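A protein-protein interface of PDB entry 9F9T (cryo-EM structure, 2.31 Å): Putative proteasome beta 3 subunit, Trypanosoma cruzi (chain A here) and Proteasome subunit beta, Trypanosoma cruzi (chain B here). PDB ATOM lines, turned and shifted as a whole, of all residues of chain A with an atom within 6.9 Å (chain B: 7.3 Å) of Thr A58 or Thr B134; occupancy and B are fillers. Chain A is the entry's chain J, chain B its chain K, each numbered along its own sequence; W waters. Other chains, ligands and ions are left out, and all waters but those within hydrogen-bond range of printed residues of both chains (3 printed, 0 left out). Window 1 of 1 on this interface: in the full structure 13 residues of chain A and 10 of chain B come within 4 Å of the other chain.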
ATOM      1  N   TYR A   6      23.395  -5.085  -1.039  1.00  0.00           N
ATOM      2  CA  TYR A   6      22.352  -4.878  -0.029  1.00  0.00           C
ATOM      3  C   TYR A   6      21.299  -3.866  -0.436  1.00  0.00           C
ATOM      4  O   TYR A   6      20.130  -4.073  -0.222  1.00  0.00           O
ATOM      5  CB  TYR A   6      22.941  -4.396   1.310  1.00  0.00           C
ATOM      6  CG  TYR A   6      21.964  -4.355   2.454  1.00  0.00           C
ATOM      7  CD1 TYR A   6      21.487  -5.540   3.040  1.00  0.00           C
ATOM      8  CD2 TYR A   6      21.508  -3.143   2.942  1.00  0.00           C
ATOM      9  CE1 TYR A   6      20.573  -5.514   4.082  1.00  0.00           C
ATOM     10  CE2 TYR A   6      20.584  -3.107   3.964  1.00  0.00           C
ATOM     11  CZ  TYR A   6      20.116  -4.289   4.534  1.00  0.00           C
ATOM     12  OH  TYR A   6      19.212  -4.193   5.559  1.00  0.00           O
ATOM     13  N   SER A   7      21.702  -2.754  -1.004  1.00  0.00           N
ATOM     14  CA  SER A   7      20.802  -1.609  -1.146  1.00  0.00           C
ATOM     15  C   SER A   7      20.188  -1.574  -2.544  1.00  0.00           C
ATOM     16  O   SER A   7      19.174  -0.960  -2.793  1.00  0.00           O
ATOM     17  CB  SER A   7      21.532  -0.291  -0.748  1.00  0.00           C
ATOM     18  OG  SER A   7      21.938  -0.318   0.631  1.00  0.00           O
ATOM     19  N   LEU A  28      15.472   1.844  -4.099  1.00  0.00           N
ATOM     20  CA  LEU A  28      16.193   1.524  -2.870  1.00  0.00           C
ATOM     21  C   LEU A  28      15.586   0.402  -2.056  1.00  0.00           C
ATOM     22  O   LEU A  28      14.421   0.396  -1.682  1.00  0.00           O
ATOM     23  CB  LEU A  28      16.125   2.737  -1.963  1.00  0.00           C
ATOM     24  CG  LEU A  28      16.783   2.597  -0.590  1.00  0.00           C
ATOM     25  CD1 LEU A  28      18.310   2.499  -0.680  1.00  0.00           C
ATOM     26  CD2 LEU A  28      16.400   3.789   0.242  1.00  0.00           C
ATOM     27  N   GLY A  29      16.465  -0.470  -1.610  1.00  0.00           N
ATOM     28  CA  GLY A  29      16.035  -1.715  -1.014  1.00  0.00           C
ATOM     29  C   GLY A  29      16.839  -2.125   0.198  1.00  0.00           C
ATOM     30  O   GLY A  29      17.826  -1.507   0.549  1.00  0.00           O
ATOM     31  N   GLU A  30      16.315  -3.166   0.859  1.00  0.00           N
ATOM     32  CA  GLU A  30      17.026  -3.971   1.835  1.00  0.00           C
ATOM     33  C   GLU A  30      16.969  -5.434   1.389  1.00  0.00           C
ATOM     34  O   GLU A  30      16.005  -6.165   1.639  1.00  0.00           O
ATOM     35  CB  GLU A  30      16.395  -3.743   3.194  1.00  0.00           C
ATOM     36  CG  GLU A  30      16.748  -2.440   3.875  1.00  0.00           C
ATOM     37  CD  GLU A  30      15.925  -2.124   5.145  1.00  0.00           C
ATOM     38  OE1 GLU A  30      15.873  -0.905   5.581  1.00  0.00           O
ATOM     39  OE2 GLU A  30      15.359  -3.102   5.752  1.00  0.00           O
ATOM     40  N   ILE A  35      12.112  -0.488  -0.109  1.00  0.00           N
ATOM     41  CA  ILE A  35      11.798   0.691   0.698  1.00  0.00           C
ATOM     42  C   ILE A  35      11.273   1.897  -0.111  1.00  0.00           C
ATOM     43  O   ILE A  35      10.352   2.584   0.336  1.00  0.00           O
ATOM     44  CB  ILE A  35      13.033   1.141   1.512  1.00  0.00           C
ATOM     45  CG1 ILE A  35      13.515   0.114   2.539  1.00  0.00           C
ATOM     46  CG2 ILE A  35      12.830   2.495   2.181  1.00  0.00           C
ATOM     47  CD1 ILE A  35      12.373  -0.634   3.231  1.00  0.00           C
ATOM     48  N   GLY A  55      26.399   0.838  -4.611  1.00  0.00           N
ATOM     49  CA  GLY A  55      26.927   0.222  -3.409  1.00  0.00           C
ATOM     50  C   GLY A  55      25.983   0.447  -2.251  1.00  0.00           C
ATOM     51  O   GLY A  55      24.855   0.850  -2.473  1.00  0.00           O
ATOM     52  N   LEU A  56      26.478   0.304  -1.028  1.00  0.00           N
ATOM     53  CA  LEU A  56      25.644   0.461   0.164  1.00  0.00           C
ATOM     54  C   LEU A  56      25.165   1.903   0.402  1.00  0.00           C
ATOM     55  O   LEU A  56      25.960   2.821   0.550  1.00  0.00           O
ATOM     56  CB  LEU A  56      26.530  -0.044   1.285  1.00  0.00           C
ATOM     57  CG  LEU A  56      25.863  -0.133   2.649  1.00  0.00           C
ATOM     58  CD1 LEU A  56      24.924  -1.296   2.676  1.00  0.00           C
ATOM     59  CD2 LEU A  56      26.897  -0.358   3.747  1.00  0.00           C
ATOM     60  N   ARG A  57      23.884   2.107   0.624  1.00  0.00           N
ATOM     61  CA  ARG A  57      23.351   3.434   0.626  1.00  0.00           C
ATOM     62  C   ARG A  57      23.901   4.260   1.795  1.00  0.00           C
ATOM     63  O   ARG A  57      24.140   5.461   1.655  1.00  0.00           O
ATOM     64  CB  ARG A  57      21.835   3.353   0.571  1.00  0.00           C
ATOM     65  CG  ARG A  57      21.068   4.694   0.636  1.00  0.00           C
ATOM     66  CD  ARG A  57      21.077   5.302  -0.706  1.00  0.00           C
ATOM     67  NE  ARG A  57      20.250   6.491  -0.797  1.00  0.00           N
ATOM     68  CZ  ARG A  57      20.590   7.531  -1.562  1.00  0.00           C
ATOM     69  NH1 ARG A  57      21.656   7.467  -2.361  1.00  0.00           N
ATOM     70  NH2 ARG A  57      19.821   8.596  -1.589  1.00  0.00           N
ATOM     71  N   THR A  58      24.095   3.717   2.993  1.00  0.00           N
ATOM     72  CA  THR A  58      24.691   4.600   3.995  1.00  0.00           C
ATOM     73  C   THR A  58      26.028   5.159   3.502  1.00  0.00           C
ATOM     74  O   THR A  58      26.325   6.343   3.721  1.00  0.00           O
ATOM     75  CB  THR A  58      24.800   3.950   5.364  1.00  0.00           C
ATOM     76  OG1 THR A  58      25.390   4.829   6.308  1.00  0.00           O
ATOM     77  CG2 THR A  58      25.718   2.757   5.397  1.00  0.00           C
ATOM     78  N   ASP A  59      26.831   4.354   2.790  1.00  0.00           N
ATOM     79  CA  ASP A  59      28.141   4.840   2.330  1.00  0.00           C
ATOM     80  C   ASP A  59      28.034   5.717   1.098  1.00  0.00           C
ATOM     81  O   ASP A  59      28.719   6.691   0.990  1.00  0.00           O
ATOM     82  CB  ASP A  59      29.070   3.675   2.027  1.00  0.00           C
ATOM     83  CG  ASP A  59      29.616   2.939   3.239  1.00  0.00           C
ATOM     84  OD1 ASP A  59      29.257   3.319   4.383  1.00  0.00           O
ATOM     85  OD2 ASP A  59      30.503   2.084   3.027  1.00  0.00           O
ATOM     86  N   GLN A  60      27.086   5.464   0.206  1.00  0.00           N
ATOM     87  CA  GLN A  60      26.790   6.495  -0.783  1.00  0.00           C
ATOM     88  C   GLN A  60      26.407   7.867  -0.227  1.00  0.00           C
ATOM     89  O   GLN A  60      26.782   8.919  -0.749  1.00  0.00           O
ATOM     90  CB  GLN A  60      25.529   6.208  -1.535  1.00  0.00           C
ATOM     91  CG  GLN A  60      25.649   4.938  -2.352  1.00  0.00           C
ATOM     92  CD  GLN A  60      24.336   4.763  -3.047  1.00  0.00           C
ATOM     93  OE1 GLN A  60      23.645   5.757  -3.284  1.00  0.00           O
ATOM     94  NE2 GLN A  60      23.930   3.502  -3.210  1.00  0.00           N
ATOM     95  N   GLN A  61      25.541   7.863   0.782  1.00  0.00           N
ATOM     96  CA  GLN A  61      25.164   9.093   1.432  1.00  0.00           C
ATOM     97  C   GLN A  61      26.361   9.741   2.105  1.00  0.00           C
ATOM     98  O   GLN A  61      26.647  10.872   1.817  1.00  0.00           O
ATOM     99  CB  GLN A  61      24.016   8.836   2.367  1.00  0.00           C
ATOM    100  CG  GLN A  61      22.769   8.477   1.620  1.00  0.00           C
ATOM    101  CD  GLN A  61      21.612   8.235   2.547  1.00  0.00           C
ATOM    102  OE1 GLN A  61      21.542   7.183   3.189  1.00  0.00           O
ATOM    103  NE2 GLN A  61      20.621   9.106   2.512  1.00  0.00           N
ATOM    104  N   THR A  62      27.154   9.012   2.847  1.00  0.00           N
ATOM    105  CA  THR A  62      28.283   9.607   3.539  1.00  0.00           C
ATOM    106  C   THR A  62      29.379  10.019   2.588  1.00  0.00           C
ATOM    107  O   THR A  62      29.988  11.023   2.794  1.00  0.00           O
ATOM    108  CB  THR A  62      28.906   8.608   4.502  1.00  0.00           C
ATOM    109  OG1 THR A  62      28.001   8.328   5.559  1.00  0.00           O
ATOM    110  CG2 THR A  62      30.168   9.097   5.151  1.00  0.00           C
ATOM    111  N   PHE A  63      29.667   9.266   1.537  1.00  0.00           N
ATOM    112  CA  PHE A  63      30.780   9.604   0.678  1.00  0.00           C
ATOM    113  C   PHE A  63      30.429  10.732  -0.258  1.00  0.00           C
ATOM    114  O   PHE A  63      31.247  11.575  -0.561  1.00  0.00           O
ATOM    115  CB  PHE A  63      31.155   8.397  -0.171  1.00  0.00           C
ATOM    116  CG  PHE A  63      32.361   8.550  -1.049  1.00  0.00           C
ATOM    117  CD1 PHE A  63      33.612   8.306  -0.541  1.00  0.00           C
ATOM    118  CD2 PHE A  63      32.227   8.949  -2.375  1.00  0.00           C
ATOM    119  CE1 PHE A  63      34.698   8.421  -1.386  1.00  0.00           C
ATOM    120  CE2 PHE A  63      33.346   9.229  -3.133  1.00  0.00           C
ATOM    121  CZ  PHE A  63      34.574   8.921  -2.648  1.00  0.00           C
ATOM    122  N   GLU A  65      28.600  13.246   0.693  1.00  0.00           N
ATOM    123  CA  GLU A  65      28.707  14.431   1.531  1.00  0.00           C
ATOM    124  C   GLU A  65      30.166  14.835   1.698  1.00  0.00           C
ATOM    125  O   GLU A  65      30.475  15.999   1.707  1.00  0.00           O
ATOM    126  CB  GLU A  65      28.018  14.175   2.876  1.00  0.00           C
ATOM    127  CG  GLU A  65      26.505  14.179   2.727  1.00  0.00           C
ATOM    128  CD  GLU A  65      25.640  13.418   3.742  1.00  0.00           C
ATOM    129  OE1 GLU A  65      26.166  12.975   4.829  1.00  0.00           O
ATOM    130  OE2 GLU A  65      24.417  13.218   3.430  1.00  0.00           O
ATOM    131  N   TRP A 103      34.981   2.350   2.023  1.00  0.00           N
ATOM    132  CA  TRP A 103      33.678   2.785   1.638  1.00  0.00           C
ATOM    133  C   TRP A 103      33.178   1.746   0.657  1.00  0.00           C
ATOM    134  O   TRP A 103      33.858   1.429  -0.318  1.00  0.00           O
ATOM    135  CB  TRP A 103      33.782   4.181   1.030  1.00  0.00           C
ATOM    136  CG  TRP A 103      34.379   5.225   1.939  1.00  0.00           C
ATOM    137  CD1 TRP A 103      35.612   5.817   1.813  1.00  0.00           C
ATOM    138  CD2 TRP A 103      33.808   5.793   3.126  1.00  0.00           C
ATOM    139  NE1 TRP A 103      35.840   6.714   2.823  1.00  0.00           N
ATOM    140  CE2 TRP A 103      34.751   6.713   3.644  1.00  0.00           C
ATOM    141  CE3 TRP A 103      32.589   5.638   3.787  1.00  0.00           C
ATOM    142  CZ2 TRP A 103      34.528   7.434   4.826  1.00  0.00           C
ATOM    143  CZ3 TRP A 103      32.355   6.351   4.949  1.00  0.00           C
ATOM    144  CH2 TRP A 103      33.317   7.233   5.467  1.00  0.00           C
ATOM    145  N   VAL A 105      31.317   1.834  -1.911  1.00  0.00           N
ATOM    146  CA  VAL A 105      30.660   2.503  -3.000  1.00  0.00           C
ATOM    147  C   VAL A 105      31.375   2.159  -4.263  1.00  0.00           C
ATOM    148  O   VAL A 105      32.575   2.007  -4.177  1.00  0.00           O
ATOM    149  CB  VAL A 105      30.641   4.019  -2.833  1.00  0.00           C
ATOM    150  CG1 VAL A 105      29.735   4.388  -1.706  1.00  0.00           C
ATOM    151  CG2 VAL A 105      32.032   4.660  -2.632  1.00  0.00           C
ATOM    152  N   ARG B  87      21.430  10.879  11.105  1.00  0.00           N
ATOM    153  CA  ARG B  87      22.066  10.044  10.132  1.00  0.00           C
ATOM    154  C   ARG B  87      23.565  10.082  10.306  1.00  0.00           C
ATOM    155  O   ARG B  87      24.172   9.038  10.266  1.00  0.00           O
ATOM    156  CB  ARG B  87      21.623  10.441   8.725  1.00  0.00           C
ATOM    157  CG  ARG B  87      21.937   9.381   7.671  1.00  0.00           C
ATOM    158  CD  ARG B  87      22.425  10.025   6.363  1.00  0.00           C
ATOM    159  NE  ARG B  87      23.830  10.249   6.207  1.00  0.00           N
ATOM    160  CZ  ARG B  87      24.686   9.263   5.981  1.00  0.00           C
ATOM    161  NH1 ARG B  87      25.982   9.488   5.953  1.00  0.00           N
ATOM    162  NH2 ARG B  87      24.259   8.039   5.853  1.00  0.00           N
ATOM    163  N   LEU B  90      24.418   7.767  13.316  1.00  0.00           N
ATOM    164  CA  LEU B  90      24.295   6.345  13.040  1.00  0.00           C
ATOM    165  C   LEU B  90      25.472   5.844  12.192  1.00  0.00           C
ATOM    166  O   LEU B  90      26.078   4.811  12.513  1.00  0.00           O
ATOM    167  CB  LEU B  90      22.977   6.085  12.351  1.00  0.00           C
ATOM    168  CG  LEU B  90      21.773   6.345  13.243  1.00  0.00           C
ATOM    169  CD1 LEU B  90      20.537   6.499  12.452  1.00  0.00           C
ATOM    170  CD2 LEU B  90      21.603   5.246  14.251  1.00  0.00           C
ATOM    171  N   ALA B  91      25.838   6.630  11.187  1.00  0.00           N
ATOM    172  CA  ALA B  91      26.890   6.308  10.255  1.00  0.00           C
ATOM    173  C   ALA B  91      28.247   6.311  10.886  1.00  0.00           C
ATOM    174  O   ALA B  91      29.035   5.451  10.520  1.00  0.00           O
ATOM    175  CB  ALA B  91      26.983   7.282   9.129  1.00  0.00           C
ATOM    176  N   GLY B  92      28.480   7.302  11.745  1.00  0.00           N
ATOM    177  CA  GLY B  92      29.711   7.426  12.512  1.00  0.00           C
ATOM    178  C   GLY B  92      29.919   6.246  13.453  1.00  0.00           C
ATOM    179  O   GLY B  92      30.951   5.583  13.459  1.00  0.00           O
ATOM    180  N   LEU B  94      28.766   3.409  13.182  1.00  0.00           N
ATOM    181  CA  LEU B  94      28.951   2.168  12.427  1.00  0.00           C
ATOM    182  C   LEU B  94      30.416   1.896  12.089  1.00  0.00           C
ATOM    183  O   LEU B  94      30.804   0.736  12.002  1.00  0.00           O
ATOM    184  CB  LEU B  94      28.067   2.179  11.166  1.00  0.00           C
ATOM    185  CG  LEU B  94      28.417   1.143  10.091  1.00  0.00           C
ATOM    186  CD1 LEU B  94      28.011  -0.247  10.537  1.00  0.00           C
ATOM    187  CD2 LEU B  94      27.769   1.483   8.752  1.00  0.00           C
ATOM    188  N   ARG B  95      31.255   2.928  11.976  1.00  0.00           N
ATOM    189  CA  ARG B  95      32.681   2.711  11.723  1.00  0.00           C
ATOM    190  C   ARG B  95      33.541   2.931  12.976  1.00  0.00           C
ATOM    191  O   ARG B  95      34.771   2.911  12.876  1.00  0.00           O
ATOM    192  CB  ARG B  95      33.148   3.633  10.574  1.00  0.00           C
ATOM    193  CG  ARG B  95      32.792   3.075   9.194  1.00  0.00           C
ATOM    194  CD  ARG B  95      33.183   3.850   7.952  1.00  0.00           C
ATOM    195  NE  ARG B  95      33.243   2.947   6.781  1.00  0.00           N
ATOM    196  CZ  ARG B  95      32.179   2.598   6.051  1.00  0.00           C
ATOM    197  NH1 ARG B  95      30.990   3.123   6.319  1.00  0.00           N
ATOM    198  NH2 ARG B  95      32.293   1.738   5.052  1.00  0.00           N
ATOM    199  N   CYS B 105      14.844   3.743  13.102  1.00  0.00           N
ATOM    200  CA  CYS B 105      14.135   4.923  13.504  1.00  0.00           C
ATOM    201  C   CYS B 105      13.162   5.391  12.439  1.00  0.00           C
ATOM    202  O   CYS B 105      13.281   5.018  11.297  1.00  0.00           O
ATOM    203  CB  CYS B 105      15.131   6.046  13.753  1.00  0.00           C
ATOM    204  SG  CYS B 105      16.449   5.703  14.958  1.00  0.00           S
ATOM    205  N   TYR B 128      12.505   7.851   7.008  1.00  0.00           N
ATOM    206  CA  TYR B 128      12.952   6.525   7.379  1.00  0.00           C
ATOM    207  C   TYR B 128      14.454   6.450   7.665  1.00  0.00           C
ATOM    208  O   TYR B 128      15.215   6.979   6.896  1.00  0.00           O
ATOM    209  CB  TYR B 128      12.703   5.727   6.088  1.00  0.00           C
ATOM    210  CG  TYR B 128      13.036   4.270   6.175  1.00  0.00           C
ATOM    211  CD1 TYR B 128      14.224   3.782   5.695  1.00  0.00           C
ATOM    212  CD2 TYR B 128      12.088   3.377   6.633  1.00  0.00           C
ATOM    213  CE1 TYR B 128      14.550   2.439   5.833  1.00  0.00           C
ATOM    214  CE2 TYR B 128      12.356   2.015   6.710  1.00  0.00           C
ATOM    215  CZ  TYR B 128      13.624   1.565   6.350  1.00  0.00           C
ATOM    216  OH  TYR B 128      13.855   0.211   6.396  1.00  0.00           O
ATOM    217  N   MET B 129      14.917   5.771   8.706  1.00  0.00           N
ATOM    218  CA  MET B 129      16.343   5.587   8.866  1.00  0.00           C
ATOM    219  C   MET B 129      16.645   4.174   9.251  1.00  0.00           C
ATOM    220  O   MET B 129      15.801   3.525   9.857  1.00  0.00           O
ATOM    221  CB  MET B 129      16.916   6.351  10.030  1.00  0.00           C
ATOM    222  CG  MET B 129      16.552   7.746   9.954  1.00  0.00           C
ATOM    223  SD  MET B 129      17.756   8.884  10.687  1.00  0.00           S
ATOM    224  CE  MET B 129      16.670  10.300  10.635  1.00  0.00           C
ATOM    225  N   ASP B 130      17.885   3.735   9.025  1.00  0.00           N
ATOM    226  CA  ASP B 130      18.225   2.430   9.547  1.00  0.00           C
ATOM    227  C   ASP B 130      19.471   2.475  10.399  1.00  0.00           C
ATOM    228  O   ASP B 130      20.153   3.463  10.498  1.00  0.00           O
ATOM    229  CB  ASP B 130      18.279   1.367   8.451  1.00  0.00           C
ATOM    230  CG  ASP B 130      19.573   1.376   7.661  1.00  0.00           C
ATOM    231  OD1 ASP B 130      20.275   2.417   7.670  1.00  0.00           O
ATOM    232  OD2 ASP B 130      19.855   0.333   7.009  1.00  0.00           O
ATOM    233  N   TYR B 131      19.749   1.382  11.047  1.00  0.00           N
ATOM    234  CA  TYR B 131      20.839   1.402  11.986  1.00  0.00           C
ATOM    235  C   TYR B 131      22.168   1.628  11.272  1.00  0.00           C
ATOM    236  O   TYR B 131      23.100   2.071  11.937  1.00  0.00           O
ATOM    237  CB  TYR B 131      20.853   0.137  12.833  1.00  0.00           C
ATOM    238  CG  TYR B 131      21.287  -1.060  12.025  1.00  0.00           C
ATOM    239  CD1 TYR B 131      20.383  -1.767  11.211  1.00  0.00           C
ATOM    240  CD2 TYR B 131      22.624  -1.448  12.077  1.00  0.00           C
ATOM    241  CE1 TYR B 131      20.830  -2.837  10.456  1.00  0.00           C
ATOM    242  CE2 TYR B 131      23.056  -2.546  11.362  1.00  0.00           C
ATOM    243  CZ  TYR B 131      22.169  -3.225  10.547  1.00  0.00           C
ATOM    244  OH  TYR B 131      22.749  -4.283   9.878  1.00  0.00           O
ATOM    245  N   LEU B 132      22.243   1.413   9.961  1.00  0.00           N
ATOM    246  CA  LEU B 132      23.466   1.688   9.212  1.00  0.00           C
ATOM    247  C   LEU B 132      23.675   3.179   8.881  1.00  0.00           C
ATOM    248  O   LEU B 132      24.784   3.616   8.587  1.00  0.00           O
ATOM    249  CB  LEU B 132      23.338   0.928   7.902  1.00  0.00           C
ATOM    250  CG  LEU B 132      23.218  -0.582   8.036  1.00  0.00           C
ATOM    251  CD1 LEU B 132      22.727  -1.240   6.728  1.00  0.00           C
ATOM    252  CD2 LEU B 132      24.572  -1.152   8.458  1.00  0.00           C
ATOM    253  N   GLY B 133      22.589   3.950   8.883  1.00  0.00           N
ATOM    254  CA  GLY B 133      22.659   5.328   8.486  1.00  0.00           C
ATOM    255  C   GLY B 133      22.006   5.583   7.158  1.00  0.00           C
ATOM    256  O   GLY B 133      22.128   6.658   6.606  1.00  0.00           O
ATOM    257  N   THR B 134      21.295   4.614   6.634  1.00  0.00           N
ATOM    258  CA  THR B 134      20.454   4.889   5.486  1.00  0.00           C
ATOM    259  C   THR B 134      19.394   5.880   5.947  1.00  0.00           C
ATOM    260  O   THR B 134      19.021   5.906   7.096  1.00  0.00           O
ATOM    261  CB  THR B 134      19.906   3.565   4.961  1.00  0.00           C
ATOM    262  OG1 THR B 134      20.992   2.632   4.974  1.00  0.00           O
ATOM    263  CG2 THR B 134      19.251   3.651   3.596  1.00  0.00           C
ATOM    264  N   MET B 135      19.010   6.792   5.090  1.00  0.00           N
ATOM    265  CA  MET B 135      18.002   7.777   5.411  1.00  0.00           C
ATOM    266  C   MET B 135      17.300   8.184   4.138  1.00  0.00           C
ATOM    267  O   MET B 135      17.973   8.538   3.204  1.00  0.00           O
ATOM    268  CB  MET B 135      18.636   9.039   5.956  1.00  0.00           C
ATOM    269  CG  MET B 135      17.706  10.170   5.837  1.00  0.00           C
ATOM    270  SD  MET B 135      18.116  11.558   6.912  1.00  0.00           S
ATOM    271  CE  MET B 135      19.037  12.679   5.852  1.00  0.00           C
ATOM    272  N   GLN B 136      15.987   8.339   4.187  1.00  0.00           N
ATOM    273  CA  GLN B 136      15.189   8.582   3.018  1.00  0.00           C
ATOM    274  C   GLN B 136      13.870   9.189   3.449  1.00  0.00           C
ATOM    275  O   GLN B 136      13.222   8.635   4.296  1.00  0.00           O
ATOM    276  CB  GLN B 136      15.011   7.231   2.324  1.00  0.00           C
ATOM    277  CG  GLN B 136      14.117   7.228   1.076  1.00  0.00           C
ATOM    278  CD  GLN B 136      14.622   8.190   0.036  1.00  0.00           C
ATOM    279  OE1 GLN B 136      15.791   8.216  -0.339  1.00  0.00           O
ATOM    280  NE2 GLN B 136      13.746   9.078  -0.355  1.00  0.00           N
HETATM  281  O   HOH W   1      22.698   1.331   3.805  1.00  0.00           O
HETATM  282  O   HOH W   2      35.530   3.693   5.166  1.00  0.00           O
HETATM  283  O   HOH W   3      18.185   7.349   0.640  1.00  0.00           O
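OE1 of Glu A30 sits at hydrogen-bond distance from OH of Tyr B128 (2.4 Å). O of Thr A58 sits at hydrogen-bond distance from NH2 of Arg B87 (3.4 Å). The side-chain hydroxyl (OG1) of Thr A58 is in hydrogen-bond range of the backbone carbonyl oxygen (O) of Leu B132 (2.7 Å). The side-chain carboxylate of Asp A59 lies within salt-bridge range of the guanidinium group of Arg B95, at 2.6 Å. NE2 of Gln A61 lies within hydrogen-bond range of O of Met B135, 2.8 Å away. The side-chain carboxylate of Glu A65 lies within salt-bridge range of the guanidinium group of Arg B87 (3.7 Å). The side-chain hydroxyl (OG1) of Thr A62 sits close to the guanidinium group (NH1) of Arg B87.
The backbone carbonyl oxygen (O) of Leu A28 sits at hydrogen-bond distance from the backbone NH (N) of Ile A35 (2.9 Å). The guanidinium group (NH1) of Arg A57 lies within hydrogen-bond range of the side-chain amide oxygen (OE1) of Gln A60, at 2.8 Å. The backbone carbonyl oxygen (O) of Arg A57 lies close to the side-chain amide oxygen (OE1) of Gln A61 (3.5 Å). N of Tyr B128 sits at hydrogen-bond distance from O of Gln B136 (2.9 Å). The side-chain carboxylate of Asp B130 sits close to the backbone NH of Leu B132 (3.2 Å). N of Thr B134 is in hydrogen-bond range of OD1 of Asp B130 (2.6 Å).
CE2 of Tyr A6 touches CD1 of Leu B132, at 3.96 Å. Ile A35 touches Tyr B128 (CD1 to OH, 3.6 Å). CG of Arg A57 touches CG2 of Thr B134, 3.6 Å away. Thr A58 touches Gly B133. Thr B134 touches Thr A58 (N to CB, 3.8 Å). NH2 of Arg B87 touches CB of Gln A61, 3.6 Å away. OE1 of Gln A61 touches O of Gly B133, 3.5 Å away. OE1 of Gln A61 touches CA of Thr B134 (3.4 Å). Ala B91 touches Thr A62 (CB to OG1, 3.9 Å). Trp A103 touches Arg B95.
Thr A58 touches just these residues of chain B: Arg B87 (3.4 Å), Leu B132 (2.7 Å), Gly B133 (3.5 Å) and Thr B134 (3.8 Å). Of chain A, only Arg A57, Thr A58 and Gln A61 come within 4 Å of Thr B134. Printed residues of chain A within 4 Å of Leu B132: Tyr A6 (3.96 Å) and Thr A58 (2.7 Å). Of the printed residues of chain B, Glu A65 touches Arg B87. The nearest residue of chain B that does not touch Thr A58 is Ala B91 (4.1 Å). The nearest printed residue of chain B that does not touch Thr A62 is Arg B95 (6.1 Å).
Hydrophobic or aromatic side chains of chain A within 4 Å of the printed part of chain B: Tyr A6, Ile A35 and Trp A103. Of the 16 printed residues of chain B, 8 touch a printed residue of chain A. Hydrophobic or aromatic side chains of chain B within 4 Å of the printed part of chain A: Ala B91, Tyr B128, Leu B132 and Met B135. Among the printed residues, 17 pairs touch across the chains.
Water W1 lies within hydrogen-bond range of the side-chain hydroxyl (OG1) of Thr B134, the backbone NH (N) of Thr A58 and the backbone NH (N) of Arg A57. Water W3 lies within hydrogen-bond range of the guanidinium group of Arg A57 (2.7 Å), the side-chain amide oxygen of Gln B136 (2.7 Å) and the backbone carbonyl oxygen of Met B135 (2.8 Å). Water W2 bridges NE of Arg B95 and N of Trp A103.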
